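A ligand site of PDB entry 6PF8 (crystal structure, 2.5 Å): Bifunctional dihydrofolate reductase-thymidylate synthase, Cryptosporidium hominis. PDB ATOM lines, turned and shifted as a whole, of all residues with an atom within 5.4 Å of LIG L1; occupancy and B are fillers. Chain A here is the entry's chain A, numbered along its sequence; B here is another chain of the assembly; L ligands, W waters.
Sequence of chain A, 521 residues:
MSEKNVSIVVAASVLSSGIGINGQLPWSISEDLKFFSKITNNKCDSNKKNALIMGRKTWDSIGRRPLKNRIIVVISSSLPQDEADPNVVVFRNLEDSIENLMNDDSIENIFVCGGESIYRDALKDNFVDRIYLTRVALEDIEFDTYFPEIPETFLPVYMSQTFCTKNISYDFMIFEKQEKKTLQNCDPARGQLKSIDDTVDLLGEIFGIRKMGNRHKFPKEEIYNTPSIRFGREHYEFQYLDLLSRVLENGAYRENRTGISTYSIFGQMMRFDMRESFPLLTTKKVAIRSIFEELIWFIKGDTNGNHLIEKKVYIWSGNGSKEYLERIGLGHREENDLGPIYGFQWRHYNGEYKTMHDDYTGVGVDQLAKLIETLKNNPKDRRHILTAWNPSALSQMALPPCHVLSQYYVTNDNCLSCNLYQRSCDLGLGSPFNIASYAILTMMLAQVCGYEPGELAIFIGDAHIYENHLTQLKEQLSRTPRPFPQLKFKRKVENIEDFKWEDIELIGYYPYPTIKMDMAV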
ATOM      1  N   ARG A 257     -25.110   0.660  -3.582  1.00  0.00           N
ATOM      2  CA  ARG A 257     -25.888  -0.526  -3.937  1.00  0.00           C
ATOM      3  C   ARG A 257     -27.377  -0.348  -3.631  1.00  0.00           C
ATOM      4  O   ARG A 257     -28.230  -0.889  -4.342  1.00  0.00           O
ATOM      5  CB  ARG A 257     -25.321  -1.744  -3.204  1.00  0.00           C
ATOM      6  CG  ARG A 257     -25.283  -1.580  -1.696  1.00  0.00           C
ATOM      7  CD  ARG A 257     -24.682  -2.794  -1.005  1.00  0.00           C
ATOM      8  NE  ARG A 257     -25.071  -2.862   0.393  1.00  0.00           N
ATOM      9  CZ  ARG A 257     -26.212  -3.391   0.825  1.00  0.00           C
ATOM     10  NH1 ARG A 257     -27.061  -3.911  -0.059  1.00  0.00           N
ATOM     11  NH2 ARG A 257     -26.503  -3.421   2.113  1.00  0.00           N
ATOM     12  N   TRP A 316     -31.749  -7.124  11.583  1.00  0.00           N
ATOM     13  CA  TRP A 316     -31.267  -7.941  10.484  1.00  0.00           C
ATOM     14  C   TRP A 316     -32.387  -8.473   9.600  1.00  0.00           C
ATOM     15  O   TRP A 316     -32.162  -9.395   8.814  1.00  0.00           O
ATOM     16  CB  TRP A 316     -30.423  -9.111  11.018  1.00  0.00           C
ATOM     17  CG  TRP A 316     -29.018  -8.712  11.368  1.00  0.00           C
ATOM     18  CD1 TRP A 316     -28.556  -8.391  12.607  1.00  0.00           C
ATOM     19  CD2 TRP A 316     -27.917  -8.581  10.473  1.00  0.00           C
ATOM     20  NE1 TRP A 316     -27.220  -8.073  12.536  1.00  0.00           N
ATOM     21  CE2 TRP A 316     -26.801  -8.184  11.230  1.00  0.00           C
ATOM     22  CE3 TRP A 316     -27.757  -8.769   9.087  1.00  0.00           C
ATOM     23  CZ2 TRP A 316     -25.547  -7.965  10.669  1.00  0.00           C
ATOM     24  CZ3 TRP A 316     -26.513  -8.555   8.533  1.00  0.00           C
ATOM     25  CH2 TRP A 316     -25.416  -8.159   9.316  1.00  0.00           C
ATOM     26  N   TYR A 342     -20.638 -12.203  10.765  1.00  0.00           N
ATOM     27  CA  TYR A 342     -20.210 -12.005  12.154  1.00  0.00           C
ATOM     28  C   TYR A 342     -20.710 -13.158  13.012  1.00  0.00           C
ATOM     29  O   TYR A 342     -21.870 -13.562  12.938  1.00  0.00           O
ATOM     30  CB  TYR A 342     -20.725 -10.687  12.737  1.00  0.00           C
ATOM     31  CG  TYR A 342     -20.658  -9.462  11.850  1.00  0.00           C
ATOM     32  CD1 TYR A 342     -19.465  -8.786  11.644  1.00  0.00           C
ATOM     33  CD2 TYR A 342     -21.817  -8.951  11.275  1.00  0.00           C
ATOM     34  CE1 TYR A 342     -19.416  -7.651  10.861  1.00  0.00           C
ATOM     35  CE2 TYR A 342     -21.779  -7.821  10.500  1.00  0.00           C
ATOM     36  CZ  TYR A 342     -20.581  -7.175  10.292  1.00  0.00           C
ATOM     37  OH  TYR A 342     -20.562  -6.041   9.507  1.00  0.00           O
ATOM     38  N   LEU A 399     -24.384 -10.063   3.690  1.00  0.00           N
ATOM     39  CA  LEU A 399     -23.747  -8.749   3.674  1.00  0.00           C
ATOM     40  C   LEU A 399     -22.302  -8.895   4.146  1.00  0.00           C
ATOM     41  O   LEU A 399     -22.049  -9.544   5.177  1.00  0.00           O
ATOM     42  CB  LEU A 399     -24.522  -7.766   4.559  1.00  0.00           C
ATOM     43  CG  LEU A 399     -24.242  -6.286   4.332  1.00  0.00           C
ATOM     44  CD1 LEU A 399     -24.566  -5.888   2.899  1.00  0.00           C
ATOM     45  CD2 LEU A 399     -25.050  -5.447   5.316  1.00  0.00           C
ATOM     46  N   PRO A 400     -21.332  -8.342   3.423  1.00  0.00           N
ATOM     47  CA  PRO A 400     -19.955  -8.418   3.889  1.00  0.00           C
ATOM     48  C   PRO A 400     -19.792  -7.664   5.184  1.00  0.00           C
ATOM     49  O   PRO A 400     -20.549  -6.718   5.474  1.00  0.00           O
ATOM     50  CB  PRO A 400     -19.165  -7.750   2.746  1.00  0.00           C
ATOM     51  CG  PRO A 400     -20.052  -7.846   1.556  1.00  0.00           C
ATOM     52  CD  PRO A 400     -21.448  -7.724   2.090  1.00  0.00           C
ATOM     53  N   CYS A 402     -19.030  -5.115   8.015  1.00  0.00           N
ATOM     54  CA  CYS A 402     -18.741  -3.686   8.100  1.00  0.00           C
ATOM     55  C   CYS A 402     -17.660  -3.401   9.131  1.00  0.00           C
ATOM     56  O   CYS A 402     -16.638  -2.790   8.803  1.00  0.00           O
ATOM     57  CB  CYS A 402     -20.020  -2.915   8.425  1.00  0.00           C
ATOM     58  SG  CYS A 402     -21.265  -3.069   7.147  1.00  0.00           S
ATOM     59  N   HIS A 403     -17.865  -3.835  10.378  1.00  0.00           N
ATOM     60  CA  HIS A 403     -16.780  -3.806  11.350  1.00  0.00           C
ATOM     61  C   HIS A 403     -15.894  -5.011  11.039  1.00  0.00           C
ATOM     62  O   HIS A 403     -16.219  -6.157  11.376  1.00  0.00           O
ATOM     63  CB  HIS A 403     -17.295  -3.802  12.784  1.00  0.00           C
ATOM     64  CG  HIS A 403     -18.461  -4.703  13.048  1.00  0.00           C
ATOM     65  ND1 HIS A 403     -18.367  -5.849  13.810  1.00  0.00           N
ATOM     66  CD2 HIS A 403     -19.772  -4.595  12.706  1.00  0.00           C
ATOM     67  CE1 HIS A 403     -19.548  -6.428  13.907  1.00  0.00           C
ATOM     68  NE2 HIS A 403     -20.418  -5.687  13.241  1.00  0.00           N
ATOM     69  N   GLN A 422     -13.553  -0.064  10.670  1.00  0.00           N
ATOM     70  CA  GLN A 422     -14.864  -0.216  10.053  1.00  0.00           C
ATOM     71  C   GLN A 422     -14.782   0.267   8.610  1.00  0.00           C
ATOM     72  O   GLN A 422     -14.485   1.436   8.367  1.00  0.00           O
ATOM     73  CB  GLN A 422     -15.922   0.569  10.842  1.00  0.00           C
ATOM     74  CG  GLN A 422     -17.353   0.346  10.413  1.00  0.00           C
ATOM     75  CD  GLN A 422     -18.327   0.985  11.392  1.00  0.00           C
ATOM     76  OE1 GLN A 422     -17.952   1.357  12.497  1.00  0.00           O
ATOM     77  NE2 GLN A 422     -19.586   1.112  10.979  1.00  0.00           N
ATOM     78  N   ARG A 423     -15.062  -0.634   7.659  1.00  0.00           N
ATOM     79  CA  ARG A 423     -14.907  -0.293   6.252  1.00  0.00           C
ATOM     80  C   ARG A 423     -16.026   0.628   5.764  1.00  0.00           C
ATOM     81  O   ARG A 423     -15.817   1.405   4.829  1.00  0.00           O
ATOM     82  CB  ARG A 423     -14.870  -1.559   5.396  1.00  0.00           C
ATOM     83  CG  ARG A 423     -16.179  -2.345   5.404  1.00  0.00           C
ATOM     84  CD  ARG A 423     -16.311  -3.256   4.208  1.00  0.00           C
ATOM     85  NE  ARG A 423     -17.583  -3.969   4.216  1.00  0.00           N
ATOM     86  CZ  ARG A 423     -18.712  -3.503   3.689  1.00  0.00           C
ATOM     87  NH1 ARG A 423     -18.719  -2.311   3.104  1.00  0.00           N
ATOM     88  NH2 ARG A 423     -19.825  -4.212   3.760  1.00  0.00           N
ATOM     89  N   SER A 424     -17.204   0.537   6.363  1.00  0.00           N
ATOM     90  CA  SER A 424     -18.361   1.301   5.919  1.00  0.00           C
ATOM     91  C   SER A 424     -19.213   1.623   7.137  1.00  0.00           C
ATOM     92  O   SER A 424     -19.512   0.719   7.925  1.00  0.00           O
ATOM     93  CB  SER A 424     -19.157   0.525   4.863  1.00  0.00           C
ATOM     94  OG  SER A 424     -20.185   1.316   4.315  1.00  0.00           O
ATOM     95  N   CYS A 425     -19.598   2.882   7.286  1.00  0.00           N
ATOM     96  CA  CYS A 425     -20.232   3.363   8.510  1.00  0.00           C
ATOM     97  C   CYS A 425     -21.496   4.148   8.180  1.00  0.00           C
ATOM     98  O   CYS A 425     -21.424   5.299   7.710  1.00  0.00           O
ATOM     99  CB  CYS A 425     -19.251   4.216   9.317  1.00  0.00           C
ATOM    100  SG  CYS A 425     -19.837   4.732  10.952  1.00  0.00           S
ATOM    101  N   ASP A 426     -22.649   3.528   8.402  1.00  0.00           N
ATOM    102  CA  ASP A 426     -23.928   4.228   8.393  1.00  0.00           C
ATOM    103  C   ASP A 426     -24.030   5.046   9.671  1.00  0.00           C
ATOM    104  O   ASP A 426     -24.354   4.527  10.737  1.00  0.00           O
ATOM    105  CB  ASP A 426     -25.067   3.215   8.277  1.00  0.00           C
ATOM    106  CG  ASP A 426     -26.439   3.863   8.248  1.00  0.00           C
ATOM    107  OD1 ASP A 426     -26.546   5.108   8.351  1.00  0.00           O
ATOM    108  OD2 ASP A 426     -27.433   3.124   8.110  1.00  0.00           O
ATOM    109  N   GLY A 430     -26.112   2.688  11.987  1.00  0.00           N
ATOM    110  CA  GLY A 430     -25.127   1.684  12.364  1.00  0.00           C
ATOM    111  C   GLY A 430     -24.124   2.177  13.385  1.00  0.00           C
ATOM    112  O   GLY A 430     -23.791   1.461  14.324  1.00  0.00           O
ATOM    113  N   SER A 431     -23.652   3.413  13.220  1.00  0.00           N
ATOM    114  CA  SER A 431     -22.558   3.906  14.068  1.00  0.00           C
ATOM    115  C   SER A 431     -22.911   3.939  15.549  1.00  0.00           C
ATOM    116  O   SER A 431     -22.090   3.467  16.351  1.00  0.00           O
ATOM    117  CB  SER A 431     -22.103   5.281  13.565  1.00  0.00           C
ATOM    118  OG  SER A 431     -20.922   5.691  14.225  1.00  0.00           O
ATOM    119  N   ASN A 434     -22.521   0.442  16.689  1.00  0.00           N
ATOM    120  CA  ASN A 434     -21.147  -0.063  16.706  1.00  0.00           C
ATOM    121  C   ASN A 434     -20.378   0.452  17.916  1.00  0.00           C
ATOM    122  O   ASN A 434     -19.586  -0.293  18.512  1.00  0.00           O
ATOM    123  CB  ASN A 434     -20.434   0.324  15.415  1.00  0.00           C
ATOM    124  CG  ASN A 434     -21.059  -0.306  14.177  1.00  0.00           C
ATOM    125  OD1 ASN A 434     -21.407   0.384  13.226  1.00  0.00           O
ATOM    126  ND2 ASN A 434     -21.169  -1.636  14.185  1.00  0.00           N
ATOM    127  N   HIS A 464     -20.489   7.852   6.084  1.00  0.00           N
ATOM    128  CA  HIS A 464     -21.494   8.459   5.218  1.00  0.00           C
ATOM    129  C   HIS A 464     -22.798   8.670   5.977  1.00  0.00           C
ATOM    130  O   HIS A 464     -23.027   8.111   7.052  1.00  0.00           O
ATOM    131  CB  HIS A 464     -21.738   7.595   3.980  1.00  0.00           C
ATOM    132  CG  HIS A 464     -22.078   6.164   4.291  1.00  0.00           C
ATOM    133  ND1 HIS A 464     -21.136   5.172   4.374  1.00  0.00           N
ATOM    134  CD2 HIS A 464     -23.271   5.574   4.544  1.00  0.00           C
ATOM    135  CE1 HIS A 464     -21.722   4.025   4.667  1.00  0.00           C
ATOM    136  NE2 HIS A 464     -23.018   4.242   4.770  1.00  0.00           N
ATOM    137  N   TYR A 466     -26.934   8.694   4.955  1.00  0.00           N
ATOM    138  CA  TYR A 466     -27.966   8.483   3.952  1.00  0.00           C
ATOM    139  C   TYR A 466     -28.863   9.714   3.854  1.00  0.00           C
ATOM    140  O   TYR A 466     -29.215  10.333   4.859  1.00  0.00           O
ATOM    141  CB  TYR A 466     -28.798   7.244   4.299  1.00  0.00           C
ATOM    142  CG  TYR A 466     -28.075   5.948   4.013  1.00  0.00           C
ATOM    143  CD1 TYR A 466     -27.372   5.273   5.003  1.00  0.00           C
ATOM    144  CD2 TYR A 466     -28.070   5.405   2.733  1.00  0.00           C
ATOM    145  CE1 TYR A 466     -26.701   4.096   4.730  1.00  0.00           C
ATOM    146  CE2 TYR A 466     -27.402   4.232   2.448  1.00  0.00           C
ATOM    147  CZ  TYR A 466     -26.725   3.576   3.454  1.00  0.00           C
ATOM    148  OH  TYR A 466     -26.056   2.403   3.168  1.00  0.00           O
ATOM    149  N   ARG B 382     -18.045   0.092  -1.717  1.00  0.00           N
ATOM    150  CA  ARG B 382     -17.475   0.327  -0.394  1.00  0.00           C
ATOM    151  C   ARG B 382     -16.765  -0.906   0.160  1.00  0.00           C
ATOM    152  O   ARG B 382     -16.709  -1.094   1.379  1.00  0.00           O
ATOM    153  CB  ARG B 382     -18.575   0.798   0.567  1.00  0.00           C
ATOM    154  CG  ARG B 382     -19.238   2.083   0.101  1.00  0.00           C
ATOM    155  CD  ARG B 382     -20.341   2.585   1.041  1.00  0.00           C
ATOM    156  NE  ARG B 382     -21.555   1.771   0.965  1.00  0.00           N
ATOM    157  CZ  ARG B 382     -22.789   2.235   1.173  1.00  0.00           C
ATOM    158  NH1 ARG B 382     -22.973   3.518   1.456  1.00  0.00           N
ATOM    159  NH2 ARG B 382     -23.828   1.421   1.089  1.00  0.00           N
ATOM    160  N   ARG B 383     -16.213  -1.758  -0.715  1.00  0.00           N
ATOM    161  CA  ARG B 383     -15.613  -3.023  -0.307  1.00  0.00           C
ATOM    162  C   ARG B 383     -14.262  -3.273  -0.966  1.00  0.00           C
ATOM    163  O   ARG B 383     -13.841  -4.438  -1.065  1.00  0.00           O
ATOM    164  CB  ARG B 383     -16.567  -4.189  -0.603  1.00  0.00           C
ATOM    165  CG  ARG B 383     -17.930  -4.031   0.040  1.00  0.00           C
ATOM    166  CD  ARG B 383     -18.954  -4.934  -0.616  1.00  0.00           C
ATOM    167  NE  ARG B 383     -20.294  -4.702  -0.083  1.00  0.00           N
ATOM    168  CZ  ARG B 383     -21.380  -5.369  -0.475  1.00  0.00           C
ATOM    169  NH1 ARG B 383     -21.286  -6.308  -1.399  1.00  0.00           N
ATOM    170  NH2 ARG B 383     -22.557  -5.089   0.065  1.00  0.00           N
HETATM  171  N1  LIG L   1     -23.547  -0.721   8.326  1.00  0.00           N
HETATM  172  C1  LIG L   1     -22.792  -0.165   9.327  1.00  0.00           C
HETATM  173  N2  LIG L   1     -22.525  -0.864  10.446  1.00  0.00           N
HETATM  174  C2  LIG L   1     -22.983  -2.112  10.621  1.00  0.00           C
HETATM  175  C3  LIG L   1     -23.772  -2.703   9.601  1.00  0.00           C
HETATM  176  C4  LIG L   1     -24.031  -1.986   8.493  1.00  0.00           C
HETATM  177  O1  LIG L   1     -22.326   0.956   9.279  1.00  0.00           O
HETATM  178  O2  LIG L   1     -22.727  -2.737  11.636  1.00  0.00           O
HETATM  179  F1  LIG L   1     -24.257  -3.963   9.733  1.00  0.00           F
HETATM  180  C5  LIG L   1     -23.927  -0.063   7.052  1.00  0.00           C
HETATM  181  C6  LIG L   1     -22.801   0.714   6.313  1.00  0.00           C
HETATM  182  C7  LIG L   1     -23.451   0.893   4.927  1.00  0.00           C
HETATM  183  C8  LIG L   1     -24.366  -0.341   4.792  1.00  0.00           C
HETATM  184  O3  LIG L   1     -24.254   2.077   4.897  1.00  0.00           O
HETATM  185  O4  LIG L   1     -24.260  -1.057   6.054  1.00  0.00           O
HETATM  186  C9  LIG L   1     -24.000  -1.216   3.585  1.00  0.00           C
HETATM  187  O5  LIG L   1     -22.663  -1.694   3.713  1.00  0.00           O
HETATM  188  P1  LIG L   1     -22.011  -1.765   2.237  1.00  0.00           P
HETATM  189  O6  LIG L   1     -22.997  -1.056   1.172  1.00  0.00           O
HETATM  190  O7  LIG L   1     -20.702  -1.070   2.240  1.00  0.00           O
HETATM  191  O8  LIG L   1     -21.794  -3.292   1.826  1.00  0.00           O
HETATM  192  N1  LG2 L   2     -27.394  -1.891   6.594  1.00  0.00           N
HETATM  193  C1  LG2 L   2     -27.387  -2.667   7.745  1.00  0.00           C
HETATM  194  O1  LG2 L   2     -27.129  -0.202  10.313  1.00  0.00           O
HETATM  195  N2  LG2 L   2     -27.209  -0.008   8.071  1.00  0.00           N
HETATM  196  C2  LG2 L   2     -27.299  -2.201   9.031  1.00  0.00           C
HETATM  197  O2  LG2 L   2     -32.699   0.242  12.703  1.00  0.00           O
HETATM  198  N3  LG2 L   2     -27.468  -4.037   7.789  1.00  0.00           N
HETATM  199  C3  LG2 L   2     -27.203  -0.730   9.207  1.00  0.00           C
HETATM  200  O3  LG2 L   2     -33.748  -1.320  15.263  1.00  0.00           O
HETATM  201  N4  LG2 L   2     -27.289   0.346   5.800  1.00  0.00           N
HETATM  202  C4  LG2 L   2     -27.304  -0.601   6.802  1.00  0.00           C
HETATM  203  O4  LG2 L   2     -34.211  -1.090  17.482  1.00  0.00           O
HETATM  204  C5  LG2 L   2     -27.331  -3.336   9.901  1.00  0.00           C
HETATM  205  N5  LG2 L   2     -31.554   0.502  14.654  1.00  0.00           N
HETATM  206  C6  LG2 L   2     -27.430  -4.447   9.112  1.00  0.00           C
HETATM  207  C7  LG2 L   2     -30.734  -1.627  11.730  1.00  0.00           C
HETATM  208  C8  LG2 L   2     -30.588  -0.842  12.896  1.00  0.00           C
HETATM  209  C9  LG2 L   2     -29.348  -0.873  13.570  1.00  0.00           C
HETATM  210  C10 LG2 L   2     -28.284  -1.669  13.105  1.00  0.00           C
HETATM  211  C11 LG2 L   2     -31.723   0.018  13.414  1.00  0.00           C
HETATM  212  C12 LG2 L   2     -32.412   1.360  15.429  1.00  0.00           C
HETATM  213  C13 LG2 L   2     -32.174   2.759  15.373  1.00  0.00           C
HETATM  214  C14 LG2 L   2     -32.969   3.664  16.097  1.00  0.00           C
HETATM  215  C15 LG2 L   2     -34.016   3.189  16.900  1.00  0.00           C
HETATM  216  C16 LG2 L   2     -34.263   1.808  16.970  1.00  0.00           C
HETATM  217  C17 LG2 L   2     -33.474   0.868  16.252  1.00  0.00           C
HETATM  218  C18 LG2 L   2     -33.842  -0.594  16.410  1.00  0.00           C
HETATM  219  C19 LG2 L   2     -27.285  -3.309  11.414  1.00  0.00           C
HETATM  220  C20 LG2 L   2     -28.430  -2.455  11.939  1.00  0.00           C
HETATM  221  C21 LG2 L   2     -29.666  -2.426  11.256  1.00  0.00           C
HETATM  222 CL1  LG2 L   2     -32.644   5.364  15.984  1.00  0.00          CL
HETATM  223  O   HOH W   1     -23.346  -5.937  12.859  1.00  0.00           O
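NE2 of Gln 422 sits close to SG of Cys 425 (3.6 Å).
The backbone NH of Ser 431 sits at hydrogen-bond distance from the backbone carbonyl oxygen of Asp 426 (2.8 Å).
The backbone carbonyl oxygen of Ser 424 is in hydrogen-bond range of the side-chain amide nitrogen of Gln 422, 3.1 Å away.
The backbone carbonyl oxygen (O) of Gly 430 sits close to the side-chain amide oxygen (OD1) of Asn 434 (2.8 Å).
The guanidinium group (NH2) of Arg 423 lies within hydrogen-bond range of the backbone carbonyl oxygen (O) of Pro 400 (3.1 Å).
The guanidinium group of Arg 423 sits at hydrogen-bond distance from the backbone carbonyl oxygen of Arg 382 of chain B (2.9 Å).
NE2 of Gln 422 is in hydrogen-bond range of OD1 of Asn 434.
The side-chain hydroxyl of Tyr 466 is in hydrogen-bond range of the guanidinium group of Arg 382 of chain B.
Water W1 lies within hydrogen-bond range of NE2 of His 403 and O2 of LIG L1.
O3 of LIG L1 is in hydrogen-bond range of OH of Tyr 466, 2.5 Å away.
The side-chain amide nitrogen (ND2) of Asn 434 sits at hydrogen-bond distance from an oxygen (O2) of LIG L1 (3.2 Å).
The guanidinium group (NH2) of Arg 382 of chain B lies within salt-bridge range of an oxygen (O6) of LIG L1 (2.6 Å).
The backbone NH (N) of Gly 430 sits close to an oxygen (O1) of LG2 L2, at 3.5 Å.
The guanidinium group (NH2) of Arg 383 of chain B lies within salt-bridge range of an oxygen (O8) of LIG L1, 2.6 Å away.
The side-chain carboxylate (OD2) of Asp 426 lies within hydrogen-bond range of a nitrogen (N2) of LG2 L2, 3.1 Å away.
An oxygen (O1) of LIG L1 sits at hydrogen-bond distance from the backbone NH of Asp 426.
An oxygen (O1) of LIG L1 sits at hydrogen-bond distance from the side-chain amide nitrogen (NE2) of Gln 422, 3.2 Å away.
NE of Arg 257 lies within salt-bridge range of O6 of LIG L1.
A ring nitrogen (NE2) of His 464 sits at hydrogen-bond distance from an oxygen (O3) of LIG L1 (2.5 Å).
The guanidinium group (NH1) of Arg 423 lies within salt-bridge range of an oxygen (O7) of LIG L1, at 2.5 Å.
SG of Cys 402 sits close to O4 of LIG L1, 3.8 Å away.
The side-chain hydroxyl of Ser 424 is in hydrogen-bond range of an oxygen (O7) of LIG L1 (3.2 Å).
An oxygen (O4) of LIG L1 sits close to a nitrogen (N4) of LG2 L2 (3.3 Å).
Merely in contact with LIG L1: Cys 425 (3.3 Å), His 403 (3.7 Å) and Leu 399 (3.9 Å).
Hydrophobic or aromatic side chains that line LIG L1: Leu 399, His 403, His 464 and Tyr 466.
Within 4 Å of LIG L1: Arg 257, Leu 399, Cys 402, His 403, Gln 422, Arg 423, Ser 424, Cys 425, Asp 426, Asn 434, His 464, Tyr 466, Arg 382 of chain B and Arg 383 of chain B.
Along chain A the residues within 4 Å of LIG L1 span positions 257 to 466.
The nearest printed residue that does not touch LIG L1 is Gly 430 (4.1 Å).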
